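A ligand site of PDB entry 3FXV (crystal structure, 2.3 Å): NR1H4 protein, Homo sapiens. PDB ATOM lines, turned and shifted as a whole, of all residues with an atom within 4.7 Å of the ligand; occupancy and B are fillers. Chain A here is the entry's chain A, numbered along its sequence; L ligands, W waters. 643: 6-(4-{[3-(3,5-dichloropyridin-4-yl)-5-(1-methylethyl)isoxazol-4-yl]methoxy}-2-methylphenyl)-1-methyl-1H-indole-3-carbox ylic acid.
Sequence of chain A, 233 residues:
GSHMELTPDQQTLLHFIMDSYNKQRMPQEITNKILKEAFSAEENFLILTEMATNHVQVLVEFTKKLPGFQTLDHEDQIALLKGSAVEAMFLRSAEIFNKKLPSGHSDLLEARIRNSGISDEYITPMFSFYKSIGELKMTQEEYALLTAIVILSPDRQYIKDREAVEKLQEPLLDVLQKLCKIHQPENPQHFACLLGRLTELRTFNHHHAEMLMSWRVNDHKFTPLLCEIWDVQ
O of Met 89 is in hydrogen-bond range of OG of Ser 93, at 3.1 Å. The side-chain hydroxyl of Thr 49 sits at hydrogen-bond distance from the backbone carbonyl oxygen of Phe 45 (3.1 Å). A ring nitrogen (ND1) of His 208 sits at hydrogen-bond distance from the side-chain hydroxyl (OH) of Tyr 122, at 2.7 Å.
The guanidinium group of Arg 92 lies within salt-bridge range of an oxygen (O12) of the ligand (2.9 Å). OH of Tyr 130 lies close to N24 of the ligand (3.0 Å). OG of Ser 93 lies within hydrogen-bond range of N24 of the ligand.
Met 26 touches the ligand (CE to C6, 3.2 Å). Phe 45 touches the ligand (CE1 to C35, 3.5 Å). O of Leu 48 touches C36 of the ligand, at 3.6 Å. Thr 49 touches the ligand. CE of Met 51 touches C3 of the ligand, 3.2 Å away. Ala 52 touches the ligand. Met 89 touches the ligand (SD to CL37, 3.5 Å). Phe 90 touches the ligand (CE1 to N24, 3.4 Å). CD1 of Ile 96 touches C38 of the ligand, 3.6 Å away. Leu 109 touches the ligand (CD2 to C38, 3.9 Å). Ile 113 touches the ligand (CG2 to CL32, 3.7 Å). Met 126 touches the ligand (SD to C23, 3.7 Å). His 208 touches the ligand. Trp 230 touches the ligand (CZ3 to C34, 3.8 Å). Hydrophobic or aromatic side chains within 4 Å of the ligand: Met 26, Phe 45, Leu 48, Met 51, Ala 52, Met 89, Phe 90, Ile 96, Leu 109, Ile 113, Met 126, His 208 and Trp 230. Of the 24 residues printed, 17 come within 4 Å of the ligand.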
ATOM      1  N   ARG A  25      10.079  -7.985 -26.332  1.00  0.00           N
ATOM      2  CA  ARG A  25      10.997  -6.955 -25.914  1.00  0.00           C
ATOM      3  C   ARG A  25      10.297  -5.607 -26.014  1.00  0.00           C
ATOM      4  O   ARG A  25       9.327  -5.420 -26.796  1.00  0.00           O
ATOM      5  CB  ARG A  25      12.242  -6.938 -26.818  1.00  0.00           C
ATOM      6  CG  ARG A  25      13.488  -7.572 -26.194  1.00  0.00           C
ATOM      7  CD  ARG A  25      14.567  -7.772 -27.240  1.00  0.00           C
ATOM      8  NE  ARG A  25      15.257  -9.087 -27.234  1.00  0.00           N
ATOM      9  CZ  ARG A  25      14.828 -10.209 -26.672  1.00  0.00           C
ATOM     10  NH1 ARG A  25      13.680 -10.271 -25.991  1.00  0.00           N
ATOM     11  NH2 ARG A  25      15.555 -11.310 -26.783  1.00  0.00           N
ATOM     12  N   MET A  26      10.824  -4.662 -25.251  1.00  0.00           N
ATOM     13  CA  MET A  26      10.379  -3.276 -25.272  1.00  0.00           C
ATOM     14  C   MET A  26      11.497  -2.543 -26.037  1.00  0.00           C
ATOM     15  O   MET A  26      12.666  -2.618 -25.644  1.00  0.00           O
ATOM     16  CB  MET A  26      10.243  -2.718 -23.838  1.00  0.00           C
ATOM     17  CG  MET A  26       9.643  -1.296 -23.726  1.00  0.00           C
ATOM     18  SD  MET A  26       7.875  -1.157 -24.248  1.00  0.00           S
ATOM     19  CE  MET A  26       7.004  -2.072 -23.094  1.00  0.00           C
ATOM     20  N   ILE A  34      11.294   6.557 -20.880  1.00  0.00           N
ATOM     21  CA  ILE A  34      10.942   6.344 -19.494  1.00  0.00           C
ATOM     22  C   ILE A  34      11.961   7.048 -18.627  1.00  0.00           C
ATOM     23  O   ILE A  34      11.625   7.629 -17.589  1.00  0.00           O
ATOM     24  CB  ILE A  34      10.871   4.853 -19.130  1.00  0.00           C
ATOM     25  CG1 ILE A  34       9.768   4.139 -19.908  1.00  0.00           C
ATOM     26  CG2 ILE A  34      10.615   4.683 -17.636  1.00  0.00           C
ATOM     27  CD1 ILE A  34       9.833   2.630 -19.732  1.00  0.00           C
ATOM     28  N   PHE A  45       1.243   9.981 -18.802  1.00  0.00           N
ATOM     29  CA  PHE A  45       0.150   9.289 -19.454  1.00  0.00           C
ATOM     30  C   PHE A  45       0.474   8.910 -20.893  1.00  0.00           C
ATOM     31  O   PHE A  45       0.090   7.816 -21.347  1.00  0.00           O
ATOM     32  CB  PHE A  45      -1.114  10.118 -19.436  1.00  0.00           C
ATOM     33  CG  PHE A  45      -2.335   9.338 -19.813  1.00  0.00           C
ATOM     34  CD1 PHE A  45      -2.966   8.490 -18.891  1.00  0.00           C
ATOM     35  CD2 PHE A  45      -2.776   9.344 -21.145  1.00  0.00           C
ATOM     36  CE1 PHE A  45      -4.062   7.743 -19.252  1.00  0.00           C
ATOM     37  CE2 PHE A  45      -3.867   8.543 -21.527  1.00  0.00           C
ATOM     38  CZ  PHE A  45      -4.519   7.765 -20.586  1.00  0.00           C
ATOM     39  N   LEU A  48       2.849   5.859 -20.888  1.00  0.00           N
ATOM     40  CA  LEU A  48       2.106   4.634 -20.607  1.00  0.00           C
ATOM     41  C   LEU A  48       1.394   4.168 -21.888  1.00  0.00           C
ATOM     42  O   LEU A  48       1.352   2.979 -22.181  1.00  0.00           O
ATOM     43  CB  LEU A  48       1.078   4.832 -19.474  1.00  0.00           C
ATOM     44  CG  LEU A  48       1.640   5.213 -18.104  1.00  0.00           C
ATOM     45  CD1 LEU A  48       0.619   4.987 -16.988  1.00  0.00           C
ATOM     46  CD2 LEU A  48       2.935   4.474 -17.855  1.00  0.00           C
ATOM     47  N   THR A  49       0.824   5.114 -22.615  1.00  0.00           N
ATOM     48  CA  THR A  49       0.137   4.873 -23.868  1.00  0.00           C
ATOM     49  C   THR A  49       1.048   4.209 -24.922  1.00  0.00           C
ATOM     50  O   THR A  49       0.684   3.248 -25.572  1.00  0.00           O
ATOM     51  CB  THR A  49      -0.468   6.177 -24.425  1.00  0.00           C
ATOM     52  OG1 THR A  49      -1.577   6.545 -23.610  1.00  0.00           O
ATOM     53  CG2 THR A  49      -0.987   5.978 -25.873  1.00  0.00           C
ATOM     54  N   MET A  51       3.818   2.555 -24.294  1.00  0.00           N
ATOM     55  CA  MET A  51       4.130   1.219 -23.774  1.00  0.00           C
ATOM     56  C   MET A  51       3.028   0.219 -24.020  1.00  0.00           C
ATOM     57  O   MET A  51       3.278  -0.916 -24.372  1.00  0.00           O
ATOM     58  CB  MET A  51       4.488   1.242 -22.294  1.00  0.00           C
ATOM     59  CG  MET A  51       5.698   2.133 -21.971  1.00  0.00           C
ATOM     60  SD  MET A  51       5.971   2.225 -20.182  1.00  0.00           S
ATOM     61  CE  MET A  51       7.208   1.015 -19.984  1.00  0.00           C
ATOM     62  N   ALA A  52       1.793   0.623 -23.730  1.00  0.00           N
ATOM     63  CA  ALA A  52       0.660  -0.263 -23.957  1.00  0.00           C
ATOM     64  C   ALA A  52       0.565  -0.699 -25.442  1.00  0.00           C
ATOM     65  O   ALA A  52       0.259  -1.853 -25.746  1.00  0.00           O
ATOM     66  CB  ALA A  52      -0.633   0.427 -23.518  1.00  0.00           C
ATOM     67  N   HIS A  55       3.335  -3.166 -26.290  1.00  0.00           N
ATOM     68  CA  HIS A  55       2.903  -4.464 -25.741  1.00  0.00           C
ATOM     69  C   HIS A  55       1.792  -5.216 -26.567  1.00  0.00           C
ATOM     70  O   HIS A  55       1.856  -6.435 -26.719  1.00  0.00           O
ATOM     71  CB  HIS A  55       2.425  -4.359 -24.280  1.00  0.00           C
ATOM     72  CG  HIS A  55       2.128  -5.697 -23.681  1.00  0.00           C
ATOM     73  ND1 HIS A  55       0.841  -6.210 -23.596  1.00  0.00           N
ATOM     74  CD2 HIS A  55       2.957  -6.712 -23.330  1.00  0.00           C
ATOM     75  CE1 HIS A  55       0.900  -7.442 -23.115  1.00  0.00           C
ATOM     76  NE2 HIS A  55       2.171  -7.751 -22.921  1.00  0.00           N
ATOM     77  N   MET A  89      -1.544  -7.562 -20.440  1.00  0.00           N
ATOM     78  CA  MET A  89      -0.747  -6.369 -20.169  1.00  0.00           C
ATOM     79  C   MET A  89      -0.475  -6.169 -18.650  1.00  0.00           C
ATOM     80  O   MET A  89       0.612  -5.745 -18.260  1.00  0.00           O
ATOM     81  CB  MET A  89      -1.394  -5.146 -20.769  1.00  0.00           C
ATOM     82  CG  MET A  89      -0.446  -3.990 -20.968  1.00  0.00           C
ATOM     83  SD  MET A  89      -1.332  -2.658 -21.702  1.00  0.00           S
ATOM     84  CE  MET A  89      -1.928  -3.445 -23.211  1.00  0.00           C
ATOM     85  N   PHE A  90      -1.454  -6.504 -17.802  1.00  0.00           N
ATOM     86  CA  PHE A  90      -1.246  -6.457 -16.348  1.00  0.00           C
ATOM     87  C   PHE A  90      -0.306  -7.588 -15.850  1.00  0.00           C
ATOM     88  O   PHE A  90       0.501  -7.404 -14.925  1.00  0.00           O
ATOM     89  CB  PHE A  90      -2.581  -6.539 -15.623  1.00  0.00           C
ATOM     90  CG  PHE A  90      -3.183  -5.196 -15.305  1.00  0.00           C
ATOM     91  CD1 PHE A  90      -2.731  -4.464 -14.210  1.00  0.00           C
ATOM     92  CD2 PHE A  90      -4.102  -4.628 -16.158  1.00  0.00           C
ATOM     93  CE1 PHE A  90      -3.250  -3.209 -13.977  1.00  0.00           C
ATOM     94  CE2 PHE A  90      -4.620  -3.385 -15.941  1.00  0.00           C
ATOM     95  CZ  PHE A  90      -4.201  -2.668 -14.852  1.00  0.00           C
ATOM     96  N   ARG A  92       2.146  -9.005 -17.557  1.00  0.00           N
ATOM     97  CA  ARG A  92       3.485  -8.693 -17.977  1.00  0.00           C
ATOM     98  C   ARG A  92       4.043  -7.577 -17.105  1.00  0.00           C
ATOM     99  O   ARG A  92       5.213  -7.625 -16.746  1.00  0.00           O
ATOM    100  CB  ARG A  92       3.472  -8.236 -19.441  1.00  0.00           C
ATOM    101  CG  ARG A  92       4.852  -7.916 -20.031  1.00  0.00           C
ATOM    102  CD  ARG A  92       5.782  -9.110 -19.923  1.00  0.00           C
ATOM    103  NE  ARG A  92       7.105  -8.821 -20.482  1.00  0.00           N
ATOM    104  CZ  ARG A  92       8.082  -9.715 -20.600  1.00  0.00           C
ATOM    105  NH1 ARG A  92       7.923 -10.939 -20.141  1.00  0.00           N
ATOM    106  NH2 ARG A  92       9.233  -9.385 -21.176  1.00  0.00           N
ATOM    107  N   SER A  93       3.195  -6.591 -16.798  1.00  0.00           N
ATOM    108  CA  SER A  93       3.596  -5.450 -15.939  1.00  0.00           C
ATOM    109  C   SER A  93       4.075  -6.018 -14.624  1.00  0.00           C
ATOM    110  O   SER A  93       5.154  -5.674 -14.143  1.00  0.00           O
ATOM    111  CB  SER A  93       2.431  -4.492 -15.652  1.00  0.00           C
ATOM    112  OG  SER A  93       2.250  -3.641 -16.745  1.00  0.00           O
ATOM    113  N   ILE A  96       7.596  -7.686 -14.913  1.00  0.00           N
ATOM    114  CA  ILE A  96       8.708  -6.778 -14.992  1.00  0.00           C
ATOM    115  C   ILE A  96       8.980  -6.052 -13.669  1.00  0.00           C
ATOM    116  O   ILE A  96      10.133  -5.895 -13.260  1.00  0.00           O
ATOM    117  CB  ILE A  96       8.619  -5.830 -16.257  1.00  0.00           C
ATOM    118  CG1 ILE A  96       7.274  -5.103 -16.308  1.00  0.00           C
ATOM    119  CG2 ILE A  96       8.748  -6.667 -17.541  1.00  0.00           C
ATOM    120  CD1 ILE A  96       7.357  -3.614 -16.073  1.00  0.00           C
ATOM    121  N   LEU A 109       9.844   4.305 -13.342  1.00  0.00           N
ATOM    122  CA  LEU A 109       8.646   3.847 -14.030  1.00  0.00           C
ATOM    123  C   LEU A 109       7.504   3.883 -13.039  1.00  0.00           C
ATOM    124  O   LEU A 109       6.468   4.491 -13.305  1.00  0.00           O
ATOM    125  CB  LEU A 109       8.820   2.456 -14.650  1.00  0.00           C
ATOM    126  CG  LEU A 109       7.546   1.801 -15.187  1.00  0.00           C
ATOM    127  CD1 LEU A 109       7.013   2.550 -16.424  1.00  0.00           C
ATOM    128  CD2 LEU A 109       7.832   0.327 -15.530  1.00  0.00           C
ATOM    129  N   ILE A 113       3.898   5.992 -13.328  1.00  0.00           N
ATOM    130  CA  ILE A 113       2.581   5.375 -13.227  1.00  0.00           C
ATOM    131  C   ILE A 113       1.755   6.087 -12.125  1.00  0.00           C
ATOM    132  O   ILE A 113       0.617   6.483 -12.360  1.00  0.00           O
ATOM    133  CB  ILE A 113       2.706   3.851 -12.992  1.00  0.00           C
ATOM    134  CG1 ILE A 113       3.367   3.172 -14.208  1.00  0.00           C
ATOM    135  CG2 ILE A 113       1.369   3.205 -12.690  1.00  0.00           C
ATOM    136  CD1 ILE A 113       3.705   1.656 -13.966  1.00  0.00           C
ATOM    137  N   ILE A 118      -3.876   9.156 -13.171  1.00  0.00           N
ATOM    138  CA  ILE A 118      -4.767   8.019 -12.993  1.00  0.00           C
ATOM    139  C   ILE A 118      -5.166   7.885 -11.522  1.00  0.00           C
ATOM    140  O   ILE A 118      -4.308   7.983 -10.636  1.00  0.00           O
ATOM    141  CB  ILE A 118      -4.163   6.717 -13.553  1.00  0.00           C
ATOM    142  CG1 ILE A 118      -3.939   6.838 -15.049  1.00  0.00           C
ATOM    143  CG2 ILE A 118      -5.062   5.538 -13.225  1.00  0.00           C
ATOM    144  CD1 ILE A 118      -3.491   5.531 -15.715  1.00  0.00           C
ATOM    145  N   TYR A 122      -7.732   2.919  -9.214  1.00  0.00           N
ATOM    146  CA  TYR A 122      -7.152   1.977 -10.161  1.00  0.00           C
ATOM    147  C   TYR A 122      -5.715   1.600  -9.747  1.00  0.00           C
ATOM    148  O   TYR A 122      -5.349   0.419  -9.710  1.00  0.00           O
ATOM    149  CB  TYR A 122      -7.151   2.661 -11.536  1.00  0.00           C
ATOM    150  CG  TYR A 122      -6.924   1.771 -12.752  1.00  0.00           C
ATOM    151  CD1 TYR A 122      -6.624   0.423 -12.626  1.00  0.00           C
ATOM    152  CD2 TYR A 122      -6.992   2.313 -14.032  1.00  0.00           C
ATOM    153  CE1 TYR A 122      -6.376  -0.360 -13.744  1.00  0.00           C
ATOM    154  CE2 TYR A 122      -6.752   1.540 -15.148  1.00  0.00           C
ATOM    155  CZ  TYR A 122      -6.448   0.218 -15.003  1.00  0.00           C
ATOM    156  OH  TYR A 122      -6.200  -0.537 -16.132  1.00  0.00           O
ATOM    157  N   MET A 126      -3.926  -2.246  -8.611  1.00  0.00           N
ATOM    158  CA  MET A 126      -2.825  -2.506  -9.529  1.00  0.00           C
ATOM    159  C   MET A 126      -1.545  -2.910  -8.802  1.00  0.00           C
ATOM    160  O   MET A 126      -0.930  -3.958  -9.061  1.00  0.00           O
ATOM    161  CB  MET A 126      -2.586  -1.221 -10.339  1.00  0.00           C
ATOM    162  CG  MET A 126      -1.432  -1.255 -11.304  1.00  0.00           C
ATOM    163  SD  MET A 126      -1.200   0.353 -12.120  1.00  0.00           S
ATOM    164  CE  MET A 126      -2.779   0.546 -13.037  1.00  0.00           C
ATOM    165  N   TYR A 130       0.599  -6.537  -8.227  1.00  0.00           N
ATOM    166  CA  TYR A 130       2.043  -6.710  -8.381  1.00  0.00           C
ATOM    167  C   TYR A 130       2.656  -7.363  -7.161  1.00  0.00           C
ATOM    168  O   TYR A 130       3.557  -8.213  -7.246  1.00  0.00           O
ATOM    169  CB  TYR A 130       2.746  -5.378  -8.599  1.00  0.00           C
ATOM    170  CG  TYR A 130       2.379  -4.710  -9.891  1.00  0.00           C
ATOM    171  CD1 TYR A 130       1.553  -5.344 -10.842  1.00  0.00           C
ATOM    172  CD2 TYR A 130       2.825  -3.437 -10.146  1.00  0.00           C
ATOM    173  CE1 TYR A 130       1.171  -4.691 -12.007  1.00  0.00           C
ATOM    174  CE2 TYR A 130       2.442  -2.799 -11.286  1.00  0.00           C
ATOM    175  CZ  TYR A 130       1.629  -3.420 -12.220  1.00  0.00           C
ATOM    176  OH  TYR A 130       1.342  -2.741 -13.355  1.00  0.00           O
ATOM    177  N   HIS A 208     -10.139  -0.975 -15.905  1.00  0.00           N
ATOM    178  CA  HIS A 208      -9.577  -0.383 -17.106  1.00  0.00           C
ATOM    179  C   HIS A 208     -10.635   0.340 -17.948  1.00  0.00           C
ATOM    180  O   HIS A 208     -10.344   1.369 -18.568  1.00  0.00           O
ATOM    181  CB  HIS A 208      -8.855  -1.432 -17.960  1.00  0.00           C
ATOM    182  CG  HIS A 208      -7.997  -0.836 -19.036  1.00  0.00           C
ATOM    183  ND1 HIS A 208      -6.739  -0.343 -18.798  1.00  0.00           N
ATOM    184  CD2 HIS A 208      -8.247  -0.609 -20.356  1.00  0.00           C
ATOM    185  CE1 HIS A 208      -6.250   0.176 -19.910  1.00  0.00           C
ATOM    186  NE2 HIS A 208      -7.150   0.030 -20.866  1.00  0.00           N
ATOM    187  N   MET A 211     -11.339   3.650 -16.393  1.00  0.00           N
ATOM    188  CA  MET A 211     -10.241   4.599 -16.612  1.00  0.00           C
ATOM    189  C   MET A 211     -10.382   5.209 -18.022  1.00  0.00           C
ATOM    190  O   MET A 211     -10.192   6.436 -18.220  1.00  0.00           O
ATOM    191  CB  MET A 211      -8.872   3.917 -16.450  1.00  0.00           C
ATOM    192  CG  MET A 211      -7.664   4.865 -16.627  1.00  0.00           C
ATOM    193  SD  MET A 211      -6.747   4.758 -18.251  1.00  0.00           S
ATOM    194  CE  MET A 211      -7.745   5.705 -19.333  1.00  0.00           C
ATOM    195  N   LEU A 226      -4.671   0.793 -29.832  1.00  0.00           N
ATOM    196  CA  LEU A 226      -5.417   0.751 -28.559  1.00  0.00           C
ATOM    197  C   LEU A 226      -6.916   1.049 -28.721  1.00  0.00           C
ATOM    198  O   LEU A 226      -7.756   0.386 -28.120  1.00  0.00           O
ATOM    199  CB  LEU A 226      -4.803   1.769 -27.585  1.00  0.00           C
ATOM    200  CG  LEU A 226      -3.388   1.468 -27.145  1.00  0.00           C
ATOM    201  CD1 LEU A 226      -3.010   2.436 -26.006  1.00  0.00           C
ATOM    202  CD2 LEU A 226      -3.302   0.002 -26.717  1.00  0.00           C
ATOM    203  N   TRP A 230      -9.710  -1.729 -27.579  1.00  0.00           N
ATOM    204  CA  TRP A 230     -10.560  -1.301 -26.468  1.00  0.00           C
ATOM    205  C   TRP A 230     -11.811  -0.508 -26.886  1.00  0.00           C
ATOM    206  O   TRP A 230     -12.421   0.147 -26.046  1.00  0.00           O
ATOM    207  CB  TRP A 230      -9.729  -0.501 -25.458  1.00  0.00           C
ATOM    208  CG  TRP A 230      -8.657  -1.328 -24.802  1.00  0.00           C
ATOM    209  CD1 TRP A 230      -8.695  -2.674 -24.538  1.00  0.00           C
ATOM    210  CD2 TRP A 230      -7.382  -0.845 -24.319  1.00  0.00           C
ATOM    211  NE1 TRP A 230      -7.505  -3.065 -23.951  1.00  0.00           N
ATOM    212  CE2 TRP A 230      -6.702  -1.966 -23.784  1.00  0.00           C
ATOM    213  CE3 TRP A 230      -6.782   0.409 -24.228  1.00  0.00           C
ATOM    214  CZ2 TRP A 230      -5.415  -1.859 -23.214  1.00  0.00           C
ATOM    215  CZ3 TRP A 230      -5.494   0.515 -23.682  1.00  0.00           C
ATOM    216  CH2 TRP A 230      -4.833  -0.604 -23.177  1.00  0.00           C
HETATM  217  C4  643 L   1       6.072  -4.507 -20.916  1.00  0.00           C
HETATM  218  C5  643 L   1       8.701  -4.546 -20.690  1.00  0.00           C
HETATM  219  C6  643 L   1       7.335  -4.039 -20.552  1.00  0.00           C
HETATM  220  C7  643 L   1       7.454  -2.814 -19.890  1.00  0.00           C
HETATM  221  C10 643 L   1       9.327  -1.423 -18.981  1.00  0.00           C
HETATM  222  C15 643 L   1       2.956  -1.445 -20.623  1.00  0.00           C
HETATM  223  C17 643 L   1       3.770  -1.116 -18.402  1.00  0.00           C
HETATM  224  C21 643 L   1      -1.559  -0.242 -17.074  1.00  0.00           C
HETATM  225  C22 643 L   1      -0.677  -0.033 -16.030  1.00  0.00           C
HETATM  226  C26 643 L   1      -1.881  -1.550 -17.411  1.00  0.00           C
HETATM  227  C28 643 L   1      -1.549   1.398 -19.046  1.00  0.00           C
HETATM  228  C1  643 L   1       4.958  -3.777 -20.630  1.00  0.00           C
HETATM  229  C2  643 L   1       5.069  -2.558 -19.964  1.00  0.00           C
HETATM  230  C3  643 L   1       6.319  -2.080 -19.610  1.00  0.00           C
HETATM  231  N8  643 L   1       8.786  -2.594 -19.652  1.00  0.00           N
HETATM  232  C9  643 L   1       9.514  -3.616 -20.126  1.00  0.00           C
HETATM  233  C11 643 L   1       9.149  -5.793 -21.315  1.00  0.00           C
HETATM  234  O12 643 L   1       8.347  -6.560 -21.791  1.00  0.00           O
HETATM  235  O13 643 L   1      10.451  -6.061 -21.383  1.00  0.00           O
HETATM  236  C14 643 L   1       1.880  -0.633 -20.348  1.00  0.00           C
HETATM  237  C16 643 L   1       3.896  -1.708 -19.653  1.00  0.00           C
HETATM  238  C18 643 L   1       2.702  -0.314 -18.129  1.00  0.00           C
HETATM  239  C19 643 L   1       1.757  -0.064 -19.102  1.00  0.00           C
HETATM  240  O20 643 L   1       0.722   0.736 -18.798  1.00  0.00           O
HETATM  241  C23 643 L   1      -0.166  -1.114 -15.355  1.00  0.00           C
HETATM  242  N24 643 L   1      -0.500  -2.330 -15.703  1.00  0.00           N
HETATM  243  C25 643 L   1      -1.327  -2.584 -16.691  1.00  0.00           C
HETATM  244  C27 643 L   1      -2.116   0.892 -17.850  1.00  0.00           C
HETATM  245  C29 643 L   1      -2.356   2.402 -19.398  1.00  0.00           C
HETATM  246  O30 643 L   1      -3.310   2.446 -18.467  1.00  0.00           O
HETATM  247  N31 643 L   1      -3.168   1.610 -17.624  1.00  0.00           N
HETATM  248 CL32 643 L   1      -0.261   1.566 -15.594  1.00  0.00          CL
HETATM  249  C33 643 L   1      -2.225   3.281 -20.604  1.00  0.00           C
HETATM  250  C34 643 L   1      -3.250   2.872 -21.646  1.00  0.00           C
HETATM  251  C35 643 L   1      -2.464   4.744 -20.219  1.00  0.00           C
HETATM  252  C36 643 L   1      -0.312   0.912 -19.761  1.00  0.00           C
HETATM  253 CL37 643 L   1      -2.974  -1.852 -18.692  1.00  0.00          CL
HETATM  254  C38 643 L   1       4.795  -1.377 -17.331  1.00  0.00           C
HETATM  255  O   HOH W   1       6.901  -6.557 -23.846  1.00  0.00           O
